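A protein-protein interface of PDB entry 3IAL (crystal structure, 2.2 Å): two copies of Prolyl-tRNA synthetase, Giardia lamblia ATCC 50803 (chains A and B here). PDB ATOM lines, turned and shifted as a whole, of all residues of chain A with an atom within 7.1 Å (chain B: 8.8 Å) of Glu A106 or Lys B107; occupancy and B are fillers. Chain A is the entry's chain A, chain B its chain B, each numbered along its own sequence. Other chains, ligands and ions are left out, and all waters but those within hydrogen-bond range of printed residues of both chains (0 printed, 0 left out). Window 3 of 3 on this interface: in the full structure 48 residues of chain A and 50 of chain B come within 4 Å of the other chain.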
ATOM      1  N   GLU A  85      32.514 -22.197 -18.799  1.00  0.00           N
ATOM      2  CA  GLU A  85      31.688 -22.050 -19.999  1.00  0.00           C
ATOM      3  C   GLU A  85      32.447 -21.432 -21.173  1.00  0.00           C
ATOM      4  O   GLU A  85      32.290 -21.872 -22.314  1.00  0.00           O
ATOM      5  CB  GLU A  85      30.447 -21.212 -19.691  1.00  0.00           C
ATOM      6  CG  GLU A  85      29.507 -21.055 -20.878  1.00  0.00           C
ATOM      7  CD  GLU A  85      28.119 -20.620 -20.476  1.00  0.00           C
ATOM      8  OE1 GLU A  85      27.989 -19.918 -19.455  1.00  0.00           O
ATOM      9  OE2 GLU A  85      27.156 -20.981 -21.183  1.00  0.00           O
ATOM     10  N   CYS A 102      25.442 -30.799 -21.499  1.00  0.00           N
ATOM     11  CA  CYS A 102      26.178 -30.203 -20.376  1.00  0.00           C
ATOM     12  C   CYS A 102      25.350 -30.059 -19.095  1.00  0.00           C
ATOM     13  O   CYS A 102      24.298 -29.418 -19.092  1.00  0.00           O
ATOM     14  CB  CYS A 102      26.749 -28.845 -20.780  1.00  0.00           C
ATOM     15  SG  CYS A 102      28.179 -28.996 -21.856  1.00  0.00           S
ATOM     16  N   PHE A 103      25.823 -30.676 -18.014  1.00  0.00           N
ATOM     17  CA  PHE A 103      25.357 -30.322 -16.676  1.00  0.00           C
ATOM     18  C   PHE A 103      26.041 -29.014 -16.312  1.00  0.00           C
ATOM     19  O   PHE A 103      27.256 -28.883 -16.480  1.00  0.00           O
ATOM     20  CB  PHE A 103      25.731 -31.375 -15.646  1.00  0.00           C
ATOM     21  CG  PHE A 103      24.995 -32.676 -15.792  1.00  0.00           C
ATOM     22  CD1 PHE A 103      23.851 -32.924 -15.058  1.00  0.00           C
ATOM     23  CD2 PHE A 103      25.477 -33.666 -16.631  1.00  0.00           C
ATOM     24  CE1 PHE A 103      23.181 -34.141 -15.169  1.00  0.00           C
ATOM     25  CE2 PHE A 103      24.823 -34.879 -16.752  1.00  0.00           C
ATOM     26  CZ  PHE A 103      23.674 -35.121 -16.016  1.00  0.00           C
ATOM     27  N   TRP A 104      25.268 -28.050 -15.820  1.00  0.00           N
ATOM     28  CA  TRP A 104      25.806 -26.736 -15.487  1.00  0.00           C
ATOM     29  C   TRP A 104      25.825 -26.496 -13.981  1.00  0.00           C
ATOM     30  O   TRP A 104      24.784 -26.439 -13.339  1.00  0.00           O
ATOM     31  CB  TRP A 104      24.996 -25.642 -16.184  1.00  0.00           C
ATOM     32  CG  TRP A 104      25.214 -25.611 -17.665  1.00  0.00           C
ATOM     33  CD1 TRP A 104      24.351 -26.040 -18.631  1.00  0.00           C
ATOM     34  CD2 TRP A 104      26.384 -25.147 -18.348  1.00  0.00           C
ATOM     35  NE1 TRP A 104      24.906 -25.861 -19.872  1.00  0.00           N
ATOM     36  CE2 TRP A 104      26.154 -25.317 -19.727  1.00  0.00           C
ATOM     37  CE3 TRP A 104      27.603 -24.596 -17.928  1.00  0.00           C
ATOM     38  CZ2 TRP A 104      27.097 -24.957 -20.692  1.00  0.00           C
ATOM     39  CZ3 TRP A 104      28.537 -24.234 -18.883  1.00  0.00           C
ATOM     40  CH2 TRP A 104      28.281 -24.419 -20.249  1.00  0.00           C
ATOM     41  N   VAL A 105      27.023 -26.367 -13.427  1.00  0.00           N
ATOM     42  CA  VAL A 105      27.204 -25.950 -12.038  1.00  0.00           C
ATOM     43  C   VAL A 105      26.994 -24.447 -11.984  1.00  0.00           C
ATOM     44  O   VAL A 105      27.714 -23.710 -12.645  1.00  0.00           O
ATOM     45  CB  VAL A 105      28.621 -26.236 -11.524  1.00  0.00           C
ATOM     46  CG1 VAL A 105      28.749 -25.771 -10.068  1.00  0.00           C
ATOM     47  CG2 VAL A 105      28.969 -27.715 -11.684  1.00  0.00           C
ATOM     48  N   GLU A 106      26.010 -23.998 -11.211  1.00  0.00           N
ATOM     49  CA  GLU A 106      25.640 -22.581 -11.191  1.00  0.00           C
ATOM     50  C   GLU A 106      25.782 -21.909  -9.836  1.00  0.00           C
ATOM     51  O   GLU A 106      25.780 -20.679  -9.767  1.00  0.00           O
ATOM     52  CB  GLU A 106      24.211 -22.409 -11.694  1.00  0.00           C
ATOM     53  CG  GLU A 106      24.021 -22.960 -13.098  1.00  0.00           C
ATOM     54  CD  GLU A 106      22.865 -22.328 -13.831  1.00  0.00           C
ATOM     55  OE1 GLU A 106      21.828 -22.057 -13.191  1.00  0.00           O
ATOM     56  OE2 GLU A 106      22.995 -22.111 -15.055  1.00  0.00           O
ATOM     57  N   LYS A 107      25.899 -22.695  -8.764  1.00  0.00           N
ATOM     58  CA  LYS A 107      26.048 -22.136  -7.424  1.00  0.00           C
ATOM     59  C   LYS A 107      27.245 -22.739  -6.698  1.00  0.00           C
ATOM     60  O   LYS A 107      27.550 -23.918  -6.854  1.00  0.00           O
ATOM     61  CB  LYS A 107      24.771 -22.350  -6.602  1.00  0.00           C
ATOM     62  CG  LYS A 107      23.571 -21.510  -7.058  1.00  0.00           C
ATOM     63  CD  LYS A 107      22.517 -21.424  -5.963  1.00  0.00           C
ATOM     64  CE  LYS A 107      21.313 -20.569  -6.369  1.00  0.00           C
ATOM     65  NZ  LYS A 107      20.326 -21.317  -7.192  1.00  0.00           N
ATOM     66  N   GLY A 108      27.935 -21.898  -5.934  1.00  0.00           N
ATOM     67  CA  GLY A 108      28.904 -22.342  -4.940  1.00  0.00           C
ATOM     68  C   GLY A 108      28.312 -22.001  -3.585  1.00  0.00           C
ATOM     69  O   GLY A 108      28.297 -20.840  -3.193  1.00  0.00           O
ATOM     70  N   GLY A 109      27.809 -23.010  -2.875  1.00  0.00           N
ATOM     71  CA  GLY A 109      27.027 -22.781  -1.661  1.00  0.00           C
ATOM     72  C   GLY A 109      25.690 -22.180  -2.056  1.00  0.00           C
ATOM     73  O   GLY A 109      25.089 -22.598  -3.050  1.00  0.00           O
ATOM     74  N   GLN A 111      25.453 -19.048  -2.976  1.00  0.00           N
ATOM     75  CA  GLN A 111      25.784 -17.935  -3.862  1.00  0.00           C
ATOM     76  C   GLN A 111      25.919 -18.394  -5.314  1.00  0.00           C
ATOM     77  O   GLN A 111      26.632 -19.355  -5.587  1.00  0.00           O
ATOM     78  CB  GLN A 111      27.097 -17.291  -3.403  1.00  0.00           C
ATOM     79  CG  GLN A 111      27.427 -15.964  -4.073  1.00  0.00           C
ATOM     80  CD  GLN A 111      26.531 -14.822  -3.619  1.00  0.00           C
ATOM     81  OE1 GLN A 111      25.995 -14.831  -2.509  1.00  0.00           O
ATOM     82  NE2 GLN A 111      26.378 -13.823  -4.479  1.00  0.00           N
ATOM     83  N   PRO A 112      25.248 -17.701  -6.256  1.00  0.00           N
ATOM     84  CA  PRO A 112      25.487 -17.981  -7.677  1.00  0.00           C
ATOM     85  C   PRO A 112      26.955 -17.791  -8.058  1.00  0.00           C
ATOM     86  O   PRO A 112      27.615 -16.888  -7.540  1.00  0.00           O
ATOM     87  CB  PRO A 112      24.617 -16.942  -8.398  1.00  0.00           C
ATOM     88  CG  PRO A 112      23.564 -16.575  -7.422  1.00  0.00           C
ATOM     89  CD  PRO A 112      24.204 -16.676  -6.068  1.00  0.00           C
ATOM     90  N   LEU A 113      27.461 -18.645  -8.943  1.00  0.00           N
ATOM     91  CA  LEU A 113      28.837 -18.525  -9.413  1.00  0.00           C
ATOM     92  C   LEU A 113      28.948 -17.401 -10.443  1.00  0.00           C
ATOM     93  O   LEU A 113      28.045 -17.206 -11.261  1.00  0.00           O
ATOM     94  CB  LEU A 113      29.319 -19.836 -10.034  1.00  0.00           C
ATOM     95  CG  LEU A 113      29.515 -21.045  -9.116  1.00  0.00           C
ATOM     96  CD1 LEU A 113      29.937 -22.244  -9.956  1.00  0.00           C
ATOM     97  CD2 LEU A 113      30.546 -20.760  -8.014  1.00  0.00           C
ATOM     98  N   GLU A 114      30.069 -16.684 -10.403  1.00  0.00           N
ATOM     99  CA  GLU A 114      30.346 -15.598 -11.346  1.00  0.00           C
ATOM    100  C   GLU A 114      30.272 -16.104 -12.788  1.00  0.00           C
ATOM    101  O   GLU A 114      29.568 -15.531 -13.618  1.00  0.00           O
ATOM    102  CB  GLU A 114      31.729 -14.991 -11.060  1.00  0.00           C
ATOM    103  CG  GLU A 114      31.972 -13.619 -11.689  1.00  0.00           C
ATOM    104  CD  GLU A 114      33.270 -12.973 -11.206  1.00  0.00           C
ATOM    105  OE1 GLU A 114      34.278 -13.702 -11.041  1.00  0.00           O
ATOM    106  OE2 GLU A 114      33.278 -11.739 -10.988  1.00  0.00           O
ATOM    107  N   GLU A 115      31.000 -17.187 -13.061  1.00  0.00           N
ATOM    108  CA  GLU A 115      30.961 -17.882 -14.351  1.00  0.00           C
ATOM    109  C   GLU A 115      30.438 -19.307 -14.147  1.00  0.00           C
ATOM    110  O   GLU A 115      30.878 -20.004 -13.230  1.00  0.00           O
ATOM    111  CB  GLU A 115      32.370 -17.938 -14.962  1.00  0.00           C
ATOM    112  CG  GLU A 115      32.424 -18.433 -16.417  1.00  0.00           C
ATOM    113  CD  GLU A 115      33.848 -18.585 -16.958  1.00  0.00           C
ATOM    114  OE1 GLU A 115      34.811 -18.611 -16.160  1.00  0.00           O
ATOM    115  OE2 GLU A 115      34.003 -18.693 -18.196  1.00  0.00           O
ATOM    116  N   ARG A 116      29.503 -19.735 -14.996  1.00  0.00           N
ATOM    117  CA  ARG A 116      29.020 -21.118 -14.968  1.00  0.00           C
ATOM    118  C   ARG A 116      30.169 -22.081 -15.220  1.00  0.00           C
ATOM    119  O   ARG A 116      31.083 -21.786 -15.985  1.00  0.00           O
ATOM    120  CB  ARG A 116      27.962 -21.366 -16.046  1.00  0.00           C
ATOM    121  CG  ARG A 116      26.649 -20.621 -15.861  1.00  0.00           C
ATOM    122  CD  ARG A 116      25.875 -20.568 -17.173  1.00  0.00           C
ATOM    123  NE  ARG A 116      24.794 -21.545 -17.252  1.00  0.00           N
ATOM    124  CZ  ARG A 116      24.295 -22.048 -18.383  1.00  0.00           C
ATOM    125  NH1 ARG A 116      24.787 -21.703 -19.571  1.00  0.00           N
ATOM    126  NH2 ARG A 116      23.301 -22.925 -18.323  1.00  0.00           N
ATOM    127  N   LEU A 117      30.107 -23.239 -14.580  1.00  0.00           N
ATOM    128  CA  LEU A 117      31.064 -24.303 -14.823  1.00  0.00           C
ATOM    129  C   LEU A 117      30.317 -25.495 -15.373  1.00  0.00           C
ATOM    130  O   LEU A 117      29.270 -25.868 -14.851  1.00  0.00           O
ATOM    131  CB  LEU A 117      31.764 -24.694 -13.522  1.00  0.00           C
ATOM    132  CG  LEU A 117      32.646 -23.644 -12.853  1.00  0.00           C
ATOM    133  CD1 LEU A 117      33.067 -24.162 -11.474  1.00  0.00           C
ATOM    134  CD2 LEU A 117      33.874 -23.297 -13.721  1.00  0.00           C
ATOM    135  N   HIS A 154      24.326 -35.125 -20.169  1.00  0.00           N
ATOM    136  CA  HIS A 154      22.979 -34.974 -19.614  1.00  0.00           C
ATOM    137  C   HIS A 154      21.887 -35.541 -20.507  1.00  0.00           C
ATOM    138  O   HIS A 154      20.955 -36.173 -20.015  1.00  0.00           O
ATOM    139  CB  HIS A 154      22.658 -33.499 -19.342  1.00  0.00           C
ATOM    140  CG  HIS A 154      21.193 -33.226 -19.204  1.00  0.00           C
ATOM    141  ND1 HIS A 154      20.480 -33.558 -18.074  1.00  0.00           N
ATOM    142  CD2 HIS A 154      20.303 -32.674 -20.060  1.00  0.00           C
ATOM    143  CE1 HIS A 154      19.214 -33.218 -18.235  1.00  0.00           C
ATOM    144  NE2 HIS A 154      19.081 -32.679 -19.434  1.00  0.00           N
ATOM    145  N   CYS B 102      29.240 -26.817  -0.899  1.00  0.00           N
ATOM    146  CA  CYS B 102      28.636 -27.553  -2.021  1.00  0.00           C
ATOM    147  C   CYS B 102      28.511 -26.740  -3.306  1.00  0.00           C
ATOM    148  O   CYS B 102      27.905 -25.665  -3.310  1.00  0.00           O
ATOM    149  CB  CYS B 102      27.250 -28.079  -1.644  1.00  0.00           C
ATOM    150  SG  CYS B 102      27.278 -29.444  -0.480  1.00  0.00           S
ATOM    151  N   PHE B 103      29.090 -27.259  -4.386  1.00  0.00           N
ATOM    152  CA  PHE B 103      28.780 -26.801  -5.738  1.00  0.00           C
ATOM    153  C   PHE B 103      27.438 -27.397  -6.131  1.00  0.00           C
ATOM    154  O   PHE B 103      27.223 -28.582  -5.912  1.00  0.00           O
ATOM    155  CB  PHE B 103      29.821 -27.294  -6.739  1.00  0.00           C
ATOM    156  CG  PHE B 103      31.132 -26.570  -6.676  1.00  0.00           C
ATOM    157  CD1 PHE B 103      31.371 -25.460  -7.491  1.00  0.00           C
ATOM    158  CD2 PHE B 103      32.141 -27.008  -5.830  1.00  0.00           C
ATOM    159  CE1 PHE B 103      32.595 -24.796  -7.451  1.00  0.00           C
ATOM    160  CE2 PHE B 103      33.369 -26.348  -5.780  1.00  0.00           C
ATOM    161  CZ  PHE B 103      33.598 -25.245  -6.591  1.00  0.00           C
ATOM    162  N   TRP B 104      26.542 -26.603  -6.716  1.00  0.00           N
ATOM    163  CA  TRP B 104      25.225 -27.114  -7.117  1.00  0.00           C
ATOM    164  C   TRP B 104      25.065 -27.121  -8.630  1.00  0.00           C
ATOM    165  O   TRP B 104      25.295 -26.106  -9.292  1.00  0.00           O
ATOM    166  CB  TRP B 104      24.090 -26.300  -6.481  1.00  0.00           C
ATOM    167  CG  TRP B 104      24.005 -26.484  -4.992  1.00  0.00           C
ATOM    168  CD1 TRP B 104      24.509 -25.656  -4.041  1.00  0.00           C
ATOM    169  CD2 TRP B 104      23.412 -27.588  -4.291  1.00  0.00           C
ATOM    170  NE1 TRP B 104      24.257 -26.161  -2.787  1.00  0.00           N
ATOM    171  CE2 TRP B 104      23.587 -27.346  -2.911  1.00  0.00           C
ATOM    172  CE3 TRP B 104      22.749 -28.755  -4.696  1.00  0.00           C
ATOM    173  CZ2 TRP B 104      23.123 -28.228  -1.927  1.00  0.00           C
ATOM    174  CZ3 TRP B 104      22.280 -29.630  -3.721  1.00  0.00           C
ATOM    175  CH2 TRP B 104      22.476 -29.363  -2.349  1.00  0.00           C
ATOM    176  N   VAL B 105      24.676 -28.282  -9.159  1.00  0.00           N
ATOM    177  CA  VAL B 105      24.252 -28.413 -10.540  1.00  0.00           C
ATOM    178  C   VAL B 105      22.752 -28.188 -10.577  1.00  0.00           C
ATOM    179  O   VAL B 105      22.006 -28.861  -9.871  1.00  0.00           O
ATOM    180  CB  VAL B 105      24.577 -29.815 -11.115  1.00  0.00           C
ATOM    181  CG1 VAL B 105      23.960 -29.984 -12.513  1.00  0.00           C
ATOM    182  CG2 VAL B 105      26.079 -30.030 -11.151  1.00  0.00           C
ATOM    183  N   GLU B 106      22.319 -27.240 -11.396  1.00  0.00           N
ATOM    184  CA  GLU B 106      20.910 -26.839 -11.442  1.00  0.00           C
ATOM    185  C   GLU B 106      20.269 -26.963 -12.815  1.00  0.00           C
ATOM    186  O   GLU B 106      19.045 -26.976 -12.915  1.00  0.00           O
ATOM    187  CB  GLU B 106      20.761 -25.406 -10.923  1.00  0.00           C
ATOM    188  CG  GLU B 106      21.385 -25.212  -9.541  1.00  0.00           C
ATOM    189  CD  GLU B 106      20.862 -23.993  -8.806  1.00  0.00           C
ATOM    190  OE1 GLU B 106      20.407 -23.038  -9.466  1.00  0.00           O
ATOM    191  OE2 GLU B 106      20.912 -23.988  -7.561  1.00  0.00           O
ATOM    192  N   LYS B 107      21.080 -27.052 -13.869  1.00  0.00           N
ATOM    193  CA  LYS B 107      20.560 -27.242 -15.217  1.00  0.00           C
ATOM    194  C   LYS B 107      21.254 -28.396 -15.918  1.00  0.00           C
ATOM    195  O   LYS B 107      22.406 -28.710 -15.620  1.00  0.00           O
ATOM    196  CB  LYS B 107      20.725 -25.969 -16.049  1.00  0.00           C
ATOM    197  CG  LYS B 107      19.865 -24.808 -15.575  1.00  0.00           C
ATOM    198  CD  LYS B 107      19.760 -23.723 -16.633  1.00  0.00           C
ATOM    199  CE  LYS B 107      19.056 -22.480 -16.092  1.00  0.00           C
ATOM    200  NZ  LYS B 107      19.918 -21.739 -15.106  1.00  0.00           N
ATOM    201  N   GLY B 108      20.524 -29.027 -16.833  1.00  0.00           N
ATOM    202  CA  GLY B 108      21.081 -29.988 -17.774  1.00  0.00           C
ATOM    203  C   GLY B 108      20.715 -29.497 -19.154  1.00  0.00           C
ATOM    204  O   GLY B 108      19.546 -29.538 -19.539  1.00  0.00           O
ATOM    205  N   GLY B 109      21.703 -29.010 -19.897  1.00  0.00           N
ATOM    206  CA  GLY B 109      21.438 -28.329 -21.156  1.00  0.00           C
ATOM    207  C   GLY B 109      20.849 -26.960 -20.869  1.00  0.00           C
ATOM    208  O   GLY B 109      21.353 -26.236 -20.009  1.00  0.00           O
ATOM    209  N   LEU B 110      19.779 -26.608 -21.577  1.00  0.00           N
ATOM    210  CA  LEU B 110      19.074 -25.343 -21.331  1.00  0.00           C
ATOM    211  C   LEU B 110      17.964 -25.450 -20.278  1.00  0.00           C
ATOM    212  O   LEU B 110      17.440 -24.430 -19.834  1.00  0.00           O
ATOM    213  CB  LEU B 110      18.506 -24.766 -22.636  1.00  0.00           C
ATOM    214  CG  LEU B 110      19.386 -23.706 -23.310  1.00  0.00           C
ATOM    215  CD1 LEU B 110      20.509 -24.351 -24.110  1.00  0.00           C
ATOM    216  CD2 LEU B 110      18.550 -22.796 -24.200  1.00  0.00           C
ATOM    217  N   GLN B 111      17.625 -26.668 -19.865  1.00  0.00           N
ATOM    218  CA  GLN B 111      16.475 -26.894 -18.990  1.00  0.00           C
ATOM    219  C   GLN B 111      16.886 -27.155 -17.530  1.00  0.00           C
ATOM    220  O   GLN B 111      17.882 -27.839 -17.281  1.00  0.00           O
ATOM    221  CB  GLN B 111      15.619 -28.043 -19.541  1.00  0.00           C
ATOM    222  CG  GLN B 111      16.283 -29.425 -19.530  1.00  0.00           C
ATOM    223  CD  GLN B 111      16.034 -30.234 -20.802  1.00  0.00           C
ATOM    224  OE1 GLN B 111      16.873 -31.045 -21.200  1.00  0.00           O
ATOM    225  NE2 GLN B 111      14.883 -30.016 -21.441  1.00  0.00           N
ATOM    226  N   PRO B 112      16.126 -26.597 -16.561  1.00  0.00           N
ATOM    227  CA  PRO B 112      16.404 -26.840 -15.142  1.00  0.00           C
ATOM    228  C   PRO B 112      16.101 -28.267 -14.702  1.00  0.00           C
ATOM    229  O   PRO B 112      15.071 -28.818 -15.081  1.00  0.00           O
ATOM    230  CB  PRO B 112      15.448 -25.875 -14.419  1.00  0.00           C
ATOM    231  CG  PRO B 112      15.018 -24.898 -15.435  1.00  0.00           C
ATOM    232  CD  PRO B 112      15.040 -25.616 -16.736  1.00  0.00           C
ATOM    233  N   LEU B 113      16.980 -28.847 -13.886  1.00  0.00           N
ATOM    234  CA  LEU B 113      16.738 -30.179 -13.334  1.00  0.00           C
ATOM    235  C   LEU B 113      15.590 -30.095 -12.331  1.00  0.00           C
ATOM    236  O   LEU B 113      15.425 -29.077 -11.659  1.00  0.00           O
ATOM    237  CB  LEU B 113      18.000 -30.741 -12.662  1.00  0.00           C
ATOM    238  CG  LEU B 113      19.272 -30.841 -13.513  1.00  0.00           C
ATOM    239  CD1 LEU B 113      20.428 -31.363 -12.677  1.00  0.00           C
ATOM    240  CD2 LEU B 113      19.054 -31.724 -14.733  1.00  0.00           C
ATOM    241  N   GLU B 114      14.790 -31.155 -12.247  1.00  0.00           N
ATOM    242  CA  GLU B 114      13.666 -31.195 -11.303  1.00  0.00           C
ATOM    243  C   GLU B 114      14.160 -31.336  -9.861  1.00  0.00           C
ATOM    244  O   GLU B 114      13.523 -30.836  -8.931  1.00  0.00           O
ATOM    245  CB  GLU B 114      12.709 -32.341 -11.640  1.00  0.00           C
ATOM    246  CG  GLU B 114      11.459 -32.380 -10.761  1.00  0.00           C
ATOM    247  CD  GLU B 114      10.409 -33.348 -11.272  1.00  0.00           C
ATOM    248  OE1 GLU B 114      10.009 -33.223 -12.453  1.00  0.00           O
ATOM    249  OE2 GLU B 114       9.979 -34.227 -10.491  1.00  0.00           O
ATOM    250  N   GLU B 115      15.277 -32.039  -9.681  1.00  0.00           N
ATOM    251  CA  GLU B 115      15.968 -32.053  -8.398  1.00  0.00           C
ATOM    252  C   GLU B 115      17.415 -31.580  -8.582  1.00  0.00           C
ATOM    253  O   GLU B 115      18.119 -32.047  -9.479  1.00  0.00           O
ATOM    254  CB  GLU B 115      15.926 -33.448  -7.773  1.00  0.00           C
ATOM    255  CG  GLU B 115      16.344 -33.459  -6.307  1.00  0.00           C
ATOM    256  CD  GLU B 115      16.335 -34.841  -5.699  1.00  0.00           C
ATOM    257  OE1 GLU B 115      16.420 -35.830  -6.453  1.00  0.00           O
ATOM    258  OE2 GLU B 115      16.252 -34.939  -4.461  1.00  0.00           O
ATOM    259  N   ARG B 116      17.849 -30.652  -7.732  1.00  0.00           N
ATOM    260  CA  ARG B 116      19.211 -30.119  -7.803  1.00  0.00           C
ATOM    261  C   ARG B 116      20.197 -31.199  -7.381  1.00  0.00           C
ATOM    262  O   ARG B 116      19.879 -32.021  -6.524  1.00  0.00           O
ATOM    263  CB  ARG B 116      19.400 -28.923  -6.870  1.00  0.00           C
ATOM    264  CG  ARG B 116      18.388 -27.808  -7.001  1.00  0.00           C
ATOM    265  CD  ARG B 116      18.471 -26.905  -5.777  1.00  0.00           C
ATOM    266  NE  ARG B 116      19.638 -26.039  -5.835  1.00  0.00           N
ATOM    267  CZ  ARG B 116      20.371 -25.647  -4.793  1.00  0.00           C
ATOM    268  NH1 ARG B 116      20.110 -26.060  -3.557  1.00  0.00           N
ATOM    269  NH2 ARG B 116      21.399 -24.836  -4.998  1.00  0.00           N
ATOM    270  N   LEU B 117      21.388 -31.179  -7.974  1.00  0.00           N
ATOM    271  CA  LEU B 117      22.432 -32.157  -7.666  1.00  0.00           C
ATOM    272  C   LEU B 117      23.663 -31.475  -7.116  1.00  0.00           C
ATOM    273  O   LEU B 117      24.198 -30.557  -7.736  1.00  0.00           O
ATOM    274  CB  LEU B 117      22.824 -32.938  -8.920  1.00  0.00           C
ATOM    275  CG  LEU B 117      21.716 -33.727  -9.625  1.00  0.00           C
ATOM    276  CD1 LEU B 117      22.289 -34.377 -10.863  1.00  0.00           C
ATOM    277  CD2 LEU B 117      21.113 -34.757  -8.692  1.00  0.00           C
ATOM    278  N   LEU B 119      27.634 -31.583  -6.203  1.00  0.00           N
ATOM    279  CA  LEU B 119      28.880 -32.298  -6.409  1.00  0.00           C
ATOM    280  C   LEU B 119      29.347 -32.735  -5.019  1.00  0.00           C
ATOM    281  O   LEU B 119      29.381 -31.920  -4.099  1.00  0.00           O
ATOM    282  CB  LEU B 119      29.928 -31.404  -7.064  1.00  0.00           C
ATOM    283  CG  LEU B 119      29.572 -30.771  -8.414  1.00  0.00           C
ATOM    284  CD1 LEU B 119      30.797 -30.058  -8.963  1.00  0.00           C
ATOM    285  CD2 LEU B 119      29.058 -31.810  -9.408  1.00  0.00           C
ATOM    286  N   HIS B 154      33.618 -25.804  -2.276  1.00  0.00           N
ATOM    287  CA  HIS B 154      33.543 -24.442  -2.812  1.00  0.00           C
ATOM    288  C   HIS B 154      34.194 -23.368  -1.945  1.00  0.00           C
ATOM    289  O   HIS B 154      34.835 -22.464  -2.479  1.00  0.00           O
ATOM    290  CB  HIS B 154      32.090 -24.031  -3.060  1.00  0.00           C
ATOM    291  CG  HIS B 154      31.906 -22.557  -3.214  1.00  0.00           C
ATOM    292  ND1 HIS B 154      32.315 -21.869  -4.336  1.00  0.00           N
ATOM    293  CD2 HIS B 154      31.370 -21.633  -2.381  1.00  0.00           C
ATOM    294  CE1 HIS B 154      32.036 -20.586  -4.189  1.00  0.00           C
ATOM    295  NE2 HIS B 154      31.456 -20.417  -3.014  1.00  0.00           N
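The backbone NH (N) of Gly A109 sits at hydrogen-bond distance from the backbone carbonyl oxygen (O) of Cys B102.
O of Lys A107 lies within hydrogen-bond range of N of Trp B104, 2.9 Å away.
The side-chain carboxylate (OE1) of Glu A106 lies within salt-bridge range of the side-chain amino group (NZ) of Lys B107, 2.7 Å away.
O of Trp B104 sits at hydrogen-bond distance from N of Glu A106 (2.9 Å).
NZ of Lys A107 is in salt-bridge range of OE2 of Glu B106, 2.8 Å away.
NE2 of His A154 sits at hydrogen-bond distance from OE1 of Gln B111, 3.3 Å away.
A ring nitrogen (NE2) of His B154 lies within hydrogen-bond range of the backbone carbonyl oxygen of Gly A108, 3.2 Å away.
A ring nitrogen (NE2) of His A154 is in hydrogen-bond range of the backbone carbonyl oxygen (O) of Gly B108, at 3.2 Å.
The backbone NH of Gly B109 sits at hydrogen-bond distance from the backbone carbonyl oxygen of Cys A102 (2.7 Å).
O of Lys B107 sits at hydrogen-bond distance from N of Trp A104, at 2.9 Å.
O of Trp A104 sits at hydrogen-bond distance from N of Glu B106, at 3.2 Å.
The backbone NH (N) of Leu A113 lies within hydrogen-bond range of the backbone carbonyl oxygen (O) of Glu A106 (2.8 Å).
The backbone carbonyl oxygen of Leu B117 is in hydrogen-bond range of the backbone NH of Val B105 (2.7 Å).
N of Leu B113 is in hydrogen-bond range of O of Glu B106 (3.0 Å).
The side-chain carboxylate of Glu A106 is in salt-bridge range of the guanidinium group of Arg A116 (2.9 Å).
The side-chain carboxylate (OE2) of Glu B106 is in salt-bridge range of the guanidinium group (NH2) of Arg B116 (2.7 Å).
N of Leu B119 is in hydrogen-bond range of O of Phe B103 (3.0 Å).
Cys A102 touches Gly B108.
CG1 of Val B105 touches CB of Phe A103, 3.9 Å away.
Trp A104 touches Val B105 (O to CA, 3.5 Å).
O of Gly B109 touches CD1 of Trp A104, at 3.3 Å.
Val A105 touches Phe B103 (CG1 to CD1, 3.7 Å).
CG2 of Val B105 touches CG2 of Val A105, 3.7 Å away.
O of Cys B102 touches O of Lys A107 (3.97 Å).
Lys A107 touches Phe B103.
CD of Lys A107 touches NH2 of Arg B116, at 3.7 Å.
Gly A108 touches Cys B102.
Glu A106 touches two residues of chain B.
Of the printed residues of chain A, Lys B107 touches Phe A103 (3.5 Å), Trp A104 (2.9 Å) and Glu A106 (2.7 Å).
Printed residues of chain A within 4 Å of Gln B111: His A154.
Of the printed residues of chain A, Leu B113 touches His A154 (3.8 Å).
Of the printed residues of chain B, Phe A103 touches Val B105 (3.9 Å) and Lys B107 (3.5 Å).
Printed residues of chain B within 4 Å of Cys A102: Gly B108 and Gly B109.
Leu A117 touches none of the printed residues of chain B.
Arg A116 touches none of the printed residues of chain B.
The nearest printed residue of chain A that does not touch Lys B107 is Arg A116 (4.004 Å).
The nearest printed residue of chain B that does not touch Gly A109 is Phe B103 (4.7 Å).
Printed residues of chain A that touch a printed residue of chain B: Cys A102, Phe A103, Trp A104, Val A105, Glu A106, Lys A107, Gly A108, Gly A109 and His A154.
Along chain A the printed residues that touch a printed residue of chain B span positions 102 to 154.
Of the 18 printed residues of chain B, 12 touch a printed residue of chain A.
Among the printed residues, Asp or Glu carboxylates within 4 Å of a Lys or Arg side-chain nitrogen of the other chain: Glu A106 with Lys B107 and Lys A107 with Glu B106.
Val A105 touches its own counterpart, Val B105.
Glu A106 touches Lys B107, and with the chains exchanged Lys A107 touches Glu B106.
Lys A107 touches Cys B102, but with the chains exchanged Cys A102 does not touch Lys B107 (4.02 Å).
Lys A107 touches Arg B116, but with the chains exchanged Arg A116 does not touch Lys B107 (4.004 Å).
16 positions are printed for both chains.
Of the 27 pairs that touch across the chains among the printed residues, 23 have their exchanged pair printed and touching as well.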
